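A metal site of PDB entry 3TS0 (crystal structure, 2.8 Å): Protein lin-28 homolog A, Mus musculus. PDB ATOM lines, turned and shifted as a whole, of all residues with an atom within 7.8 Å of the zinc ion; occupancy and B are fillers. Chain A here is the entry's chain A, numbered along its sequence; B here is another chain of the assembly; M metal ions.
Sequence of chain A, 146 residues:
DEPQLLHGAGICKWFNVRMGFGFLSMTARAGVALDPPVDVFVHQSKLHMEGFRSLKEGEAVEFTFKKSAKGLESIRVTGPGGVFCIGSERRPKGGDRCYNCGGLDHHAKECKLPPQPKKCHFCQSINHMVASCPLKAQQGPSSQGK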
ATOM      1  N   PHE A  84      21.736   6.964 -18.858  1.00  0.00           N
ATOM      2  CA  PHE A  84      22.351   5.809 -18.204  1.00  0.00           C
ATOM      3  C   PHE A  84      23.651   6.173 -17.528  1.00  0.00           C
ATOM      4  O   PHE A  84      24.338   7.112 -17.960  1.00  0.00           O
ATOM      5  CB  PHE A  84      22.606   4.688 -19.205  1.00  0.00           C
ATOM      6  CG  PHE A  84      21.399   4.155 -19.957  1.00  0.00           C
ATOM      7  CD1 PHE A  84      20.385   3.471 -19.284  1.00  0.00           C
ATOM      8  CD2 PHE A  84      21.309   4.271 -21.334  1.00  0.00           C
ATOM      9  CE1 PHE A  84      19.293   2.959 -19.986  1.00  0.00           C
ATOM     10  CE2 PHE A  84      20.201   3.760 -22.030  1.00  0.00           C
ATOM     11  CZ  PHE A  84      19.209   3.101 -21.354  1.00  0.00           C
ATOM     12  N   ARG A  97      29.426   4.391 -25.820  1.00  0.00           N
ATOM     13  CA  ARG A  97      28.116   4.931 -25.447  1.00  0.00           C
ATOM     14  C   ARG A  97      27.647   6.057 -26.387  1.00  0.00           C
ATOM     15  O   ARG A  97      28.470   6.838 -26.838  1.00  0.00           O
ATOM     16  CB  ARG A  97      28.171   5.500 -24.009  1.00  0.00           C
ATOM     17  CG  ARG A  97      28.939   4.629 -23.019  1.00  0.00           C
ATOM     18  CD  ARG A  97      28.874   5.159 -21.595  1.00  0.00           C
ATOM     19  NE  ARG A  97      29.585   6.411 -21.373  1.00  0.00           N
ATOM     20  CZ  ARG A  97      30.897   6.523 -21.191  1.00  0.00           C
ATOM     21  NH1 ARG A  97      31.678   5.443 -21.222  1.00  0.00           N
ATOM     22  NH2 ARG A  97      31.451   7.717 -20.996  1.00  0.00           N
ATOM     23  N   CYS A  98      26.330   6.170 -26.631  1.00  0.00           N
ATOM     24  CA  CYS A  98      25.737   7.272 -27.392  1.00  0.00           C
ATOM     25  C   CYS A  98      25.993   8.611 -26.638  1.00  0.00           C
ATOM     26  O   CYS A  98      25.932   8.641 -25.404  1.00  0.00           O
ATOM     27  CB  CYS A  98      24.251   7.035 -27.598  1.00  0.00           C
ATOM     28  SG  CYS A  98      23.303   8.551 -27.872  1.00  0.00           S
ATOM     29  N   TYR A  99      26.305   9.700 -27.371  1.00  0.00           N
ATOM     30  CA  TYR A  99      26.645  10.981 -26.725  1.00  0.00           C
ATOM     31  C   TYR A  99      25.500  11.617 -25.980  1.00  0.00           C
ATOM     32  O   TYR A  99      25.744  12.320 -25.006  1.00  0.00           O
ATOM     33  CB  TYR A  99      27.227  12.003 -27.725  1.00  0.00           C
ATOM     34  CG  TYR A  99      28.577  11.652 -28.335  1.00  0.00           C
ATOM     35  CD1 TYR A  99      29.566  11.041 -27.582  1.00  0.00           C
ATOM     36  CD2 TYR A  99      28.889  12.027 -29.643  1.00  0.00           C
ATOM     37  CE1 TYR A  99      30.812  10.738 -28.134  1.00  0.00           C
ATOM     38  CE2 TYR A  99      30.122  11.744 -30.201  1.00  0.00           C
ATOM     39  CZ  TYR A  99      31.089  11.083 -29.446  1.00  0.00           C
ATOM     40  OH  TYR A  99      32.321  10.819 -29.992  1.00  0.00           O
ATOM     41  N   ASN A 100      24.250  11.370 -26.441  1.00  0.00           N
ATOM     42  CA  ASN A 100      23.015  11.938 -25.895  1.00  0.00           C
ATOM     43  C   ASN A 100      22.446  11.178 -24.707  1.00  0.00           C
ATOM     44  O   ASN A 100      22.022  11.829 -23.762  1.00  0.00           O
ATOM     45  CB  ASN A 100      21.977  12.067 -26.998  1.00  0.00           C
ATOM     46  CG  ASN A 100      20.894  13.074 -26.739  1.00  0.00           C
ATOM     47  OD1 ASN A 100      21.153  14.267 -26.632  1.00  0.00           O
ATOM     48  ND2 ASN A 100      19.642  12.636 -26.770  1.00  0.00           N
ATOM     49  N   CYS A 101      22.403   9.827 -24.742  1.00  0.00           N
ATOM     50  CA  CYS A 101      21.814   9.012 -23.675  1.00  0.00           C
ATOM     51  C   CYS A 101      22.790   8.066 -22.981  1.00  0.00           C
ATOM     52  O   CYS A 101      22.509   7.619 -21.866  1.00  0.00           O
ATOM     53  CB  CYS A 101      20.593   8.251 -24.180  1.00  0.00           C
ATOM     54  SG  CYS A 101      20.959   7.019 -25.446  1.00  0.00           S
ATOM     55  N   GLY A 102      23.901   7.752 -23.623  1.00  0.00           N
ATOM     56  CA  GLY A 102      24.892   6.867 -23.031  1.00  0.00           C
ATOM     57  C   GLY A 102      24.593   5.396 -23.233  1.00  0.00           C
ATOM     58  O   GLY A 102      25.239   4.547 -22.608  1.00  0.00           O
ATOM     59  N   GLY A 103      23.610   5.106 -24.082  1.00  0.00           N
ATOM     60  CA  GLY A 103      23.214   3.749 -24.412  1.00  0.00           C
ATOM     61  C   GLY A 103      24.308   3.053 -25.196  1.00  0.00           C
ATOM     62  O   GLY A 103      25.017   3.715 -25.959  1.00  0.00           O
ATOM     63  N   LEU A 104      24.445   1.716 -25.011  1.00  0.00           N
ATOM     64  CA  LEU A 104      25.489   0.900 -25.676  1.00  0.00           C
ATOM     65  C   LEU A 104      25.089   0.377 -27.037  1.00  0.00           C
ATOM     66  O   LEU A 104      25.968  -0.030 -27.808  1.00  0.00           O
ATOM     67  CB  LEU A 104      25.966  -0.261 -24.771  1.00  0.00           C
ATOM     68  CG  LEU A 104      26.324   0.048 -23.285  1.00  0.00           C
ATOM     69  CD1 LEU A 104      26.491  -1.225 -22.498  1.00  0.00           C
ATOM     70  CD2 LEU A 104      27.588   0.896 -23.146  1.00  0.00           C
ATOM     71  N   ASP A 105      23.785   0.430 -27.360  1.00  0.00           N
ATOM     72  CA  ASP A 105      23.154  -0.094 -28.595  1.00  0.00           C
ATOM     73  C   ASP A 105      23.350   0.718 -29.873  1.00  0.00           C
ATOM     74  O   ASP A 105      23.111   0.175 -30.947  1.00  0.00           O
ATOM     75  CB  ASP A 105      21.610  -0.207 -28.374  1.00  0.00           C
ATOM     76  CG  ASP A 105      21.115  -1.473 -27.706  1.00  0.00           C
ATOM     77  OD1 ASP A 105      21.060  -2.513 -28.386  1.00  0.00           O
ATOM     78  OD2 ASP A 105      20.723  -1.399 -26.515  1.00  0.00           O
ATOM     79  N   HIS A 106      23.633   2.045 -29.777  1.00  0.00           N
ATOM     80  CA  HIS A 106      23.686   2.951 -30.929  1.00  0.00           C
ATOM     81  C   HIS A 106      24.513   4.238 -30.629  1.00  0.00           C
ATOM     82  O   HIS A 106      25.277   4.263 -29.667  1.00  0.00           O
ATOM     83  CB  HIS A 106      22.251   3.359 -31.309  1.00  0.00           C
ATOM     84  CG  HIS A 106      21.582   4.134 -30.217  1.00  0.00           C
ATOM     85  ND1 HIS A 106      21.257   3.538 -29.011  1.00  0.00           N
ATOM     86  CD2 HIS A 106      21.328   5.459 -30.128  1.00  0.00           C
ATOM     87  CE1 HIS A 106      20.784   4.512 -28.236  1.00  0.00           C
ATOM     88  NE2 HIS A 106      20.819   5.687 -28.871  1.00  0.00           N
ATOM     89  N   HIS A 107      24.332   5.278 -31.485  1.00  0.00           N
ATOM     90  CA  HIS A 107      24.997   6.578 -31.455  1.00  0.00           C
ATOM     91  C   HIS A 107      24.004   7.725 -31.660  1.00  0.00           C
ATOM     92  O   HIS A 107      22.893   7.503 -32.167  1.00  0.00           O
ATOM     93  CB  HIS A 107      26.102   6.641 -32.534  1.00  0.00           C
ATOM     94  CG  HIS A 107      27.379   5.913 -32.210  1.00  0.00           C
ATOM     95  ND1 HIS A 107      28.450   5.901 -33.107  1.00  0.00           N
ATOM     96  CD2 HIS A 107      27.744   5.210 -31.110  1.00  0.00           C
ATOM     97  CE1 HIS A 107      29.413   5.200 -32.529  1.00  0.00           C
ATOM     98  NE2 HIS A 107      29.043   4.765 -31.326  1.00  0.00           N
ATOM     99  N   ALA A 108      24.415   8.950 -31.281  1.00  0.00           N
ATOM    100  CA  ALA A 108      23.686  10.227 -31.284  1.00  0.00           C
ATOM    101  C   ALA A 108      22.831  10.548 -32.511  1.00  0.00           C
ATOM    102  O   ALA A 108      21.809  11.219 -32.348  1.00  0.00           O
ATOM    103  CB  ALA A 108      24.613  11.377 -30.954  1.00  0.00           C
ATOM    104  N   LYS A 109      23.222  10.092 -33.709  1.00  0.00           N
ATOM    105  CA  LYS A 109      22.447  10.329 -34.938  1.00  0.00           C
ATOM    106  C   LYS A 109      21.147   9.503 -34.888  1.00  0.00           C
ATOM    107  O   LYS A 109      20.080  10.004 -35.296  1.00  0.00           O
ATOM    108  CB  LYS A 109      23.297   9.920 -36.177  1.00  0.00           C
ATOM    109  CG  LYS A 109      22.622  10.037 -37.541  1.00  0.00           C
ATOM    110  CD  LYS A 109      23.269   9.140 -38.617  1.00  0.00           C
ATOM    111  CE  LYS A 109      22.339   8.942 -39.806  1.00  0.00           C
ATOM    112  NZ  LYS A 109      22.543   7.638 -40.490  1.00  0.00           N
ATOM    113  N   GLU A 110      21.252   8.237 -34.433  1.00  0.00           N
ATOM    114  CA  GLU A 110      20.152   7.275 -34.371  1.00  0.00           C
ATOM    115  C   GLU A 110      19.382   7.295 -33.056  1.00  0.00           C
ATOM    116  O   GLU A 110      18.434   6.520 -32.895  1.00  0.00           O
ATOM    117  CB  GLU A 110      20.614   5.835 -34.702  1.00  0.00           C
ATOM    118  CG  GLU A 110      21.457   5.684 -35.961  1.00  0.00           C
ATOM    119  CD  GLU A 110      22.952   5.799 -35.691  1.00  0.00           C
ATOM    120  OE1 GLU A 110      23.463   5.015 -34.853  1.00  0.00           O
ATOM    121  OE2 GLU A 110      23.605   6.656 -36.319  1.00  0.00           O
ATOM    122  N   CYS A 111      19.779   8.179 -32.107  1.00  0.00           N
ATOM    123  CA  CYS A 111      19.146   8.352 -30.790  1.00  0.00           C
ATOM    124  C   CYS A 111      17.791   9.041 -31.036  1.00  0.00           C
ATOM    125  O   CYS A 111      17.748  10.015 -31.797  1.00  0.00           O
ATOM    126  CB  CYS A 111      20.046   9.200 -29.884  1.00  0.00           C
ATOM    127  SG  CYS A 111      19.611   9.142 -28.142  1.00  0.00           S
ATOM    128  N   LYS A 112      16.693   8.488 -30.460  1.00  0.00           N
ATOM    129  CA  LYS A 112      15.345   9.029 -30.676  1.00  0.00           C
ATOM    130  C   LYS A 112      14.775   9.840 -29.499  1.00  0.00           C
ATOM    131  O   LYS A 112      13.666  10.409 -29.599  1.00  0.00           O
ATOM    132  CB  LYS A 112      14.363   7.939 -31.157  1.00  0.00           C
ATOM    133  CG  LYS A 112      14.074   8.002 -32.667  1.00  0.00           C
ATOM    134  CD  LYS A 112      12.969   9.010 -33.003  1.00  0.00           C
ATOM    135  CE  LYS A 112      12.586   8.978 -34.466  1.00  0.00           C
ATOM    136  NZ  LYS A 112      11.278   9.658 -34.715  1.00  0.00           N
ATOM    137  N   LEU A 113      15.530   9.893 -28.407  1.00  0.00           N
ATOM    138  CA  LEU A 113      15.200  10.648 -27.209  1.00  0.00           C
ATOM    139  C   LEU A 113      15.399  12.155 -27.475  1.00  0.00           C
ATOM    140  O   LEU A 113      16.222  12.497 -28.328  1.00  0.00           O
ATOM    141  CB  LEU A 113      16.151  10.207 -26.093  1.00  0.00           C
ATOM    142  CG  LEU A 113      15.677   9.074 -25.194  1.00  0.00           C
ATOM    143  CD1 LEU A 113      16.834   8.407 -24.585  1.00  0.00           C
ATOM    144  CD2 LEU A 113      14.806   9.618 -24.033  1.00  0.00           C
ATOM    145  N   GLN A 116      19.666  16.201 -25.285  1.00  0.00           N
ATOM    146  CA  GLN A 116      20.054  16.411 -23.910  1.00  0.00           C
ATOM    147  C   GLN A 116      21.124  17.475 -23.800  1.00  0.00           C
ATOM    148  O   GLN A 116      21.842  17.704 -24.775  1.00  0.00           O
ATOM    149  CB  GLN A 116      20.589  15.094 -23.333  1.00  0.00           C
ATOM    150  CG  GLN A 116      19.611  13.925 -23.361  1.00  0.00           C
ATOM    151  CD  GLN A 116      18.428  14.071 -22.458  1.00  0.00           C
ATOM    152  OE1 GLN A 116      18.538  14.468 -21.274  1.00  0.00           O
ATOM    153  NE2 GLN A 116      17.250  13.722 -23.000  1.00  0.00           N
ATOM    154  P     G B  23      31.460  12.532 -36.503  1.00  0.00           P
ATOM    155  OP1   G B  23      32.377  12.651 -37.662  1.00  0.00           O
ATOM    156  OP2   G B  23      30.179  11.803 -36.694  1.00  0.00           O
ATOM    157  O5'   G B  23      32.271  11.844 -35.284  1.00  0.00           O
ATOM    158  C5'   G B  23      33.474  11.066 -35.487  1.00  0.00           C
ATOM    159  C4'   G B  23      33.537   9.753 -34.719  1.00  0.00           C
ATOM    160  O4'   G B  23      32.846   9.868 -33.446  1.00  0.00           O
ATOM    161  C3'   G B  23      32.912   8.536 -35.407  1.00  0.00           C
ATOM    162  O3'   G B  23      33.931   7.872 -36.151  1.00  0.00           O
ATOM    163  C2'   G B  23      32.439   7.653 -34.252  1.00  0.00           C
ATOM    164  O2'   G B  23      33.429   6.708 -33.873  1.00  0.00           O
ATOM    165  C1'   G B  23      32.218   8.646 -33.110  1.00  0.00           C
ATOM    166  N9    G B  23      30.836   8.870 -32.651  1.00  0.00           N
ATOM    167  C8    G B  23      29.823   9.541 -33.289  1.00  0.00           C
ATOM    168  N7    G B  23      28.695   9.558 -32.633  1.00  0.00           N
ATOM    169  C5    G B  23      28.984   8.878 -31.460  1.00  0.00           C
ATOM    170  C6    G B  23      28.191   8.639 -30.313  1.00  0.00           C
ATOM    171  O6    G B  23      27.020   8.972 -30.114  1.00  0.00           O
ATOM    172  N1    G B  23      28.864   7.926 -29.329  1.00  0.00           N
ATOM    173  C2    G B  23      30.183   7.531 -29.407  1.00  0.00           C
ATOM    174  N2    G B  23      30.687   6.858 -28.369  1.00  0.00           N
ATOM    175  N3    G B  23      30.936   7.773 -30.468  1.00  0.00           N
ATOM    176  C4    G B  23      30.300   8.462 -31.448  1.00  0.00           C
HETATM  177 ZN    ZN M   1      21.083   7.702 -27.499  1.00  0.00          ZN
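ND2 of Asn 100 sits close to SG of Cys 111 (3.8 Å).
N of Gly 103 lies close to SG of Cys 101 (3.5 Å).
The backbone carbonyl oxygen of Cys 101 sits at hydrogen-bond distance from the backbone NH of Phe 84 (3.2 Å).
The side-chain sulfur (SG) of Cys 98 sits close to the backbone NH (N) of Asn 100 (3.3 Å).
N of Cys 98 sits at hydrogen-bond distance from O of Gly 103 (2.9 Å).
SG of Cys 98 lies close to N of Ala 108 (3.6 Å).
The zinc ion is bound by the side-chain sulfur of Cys 111 (2.2 Å), the side-chain sulfur of Cys 101 (2.2 Å), the side-chain sulfur of Cys 98 (2.4 Å) and a ring nitrogen (NE2) of His 106 (2.5 Å).
The zinc ion has four donor atoms within binding distance.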
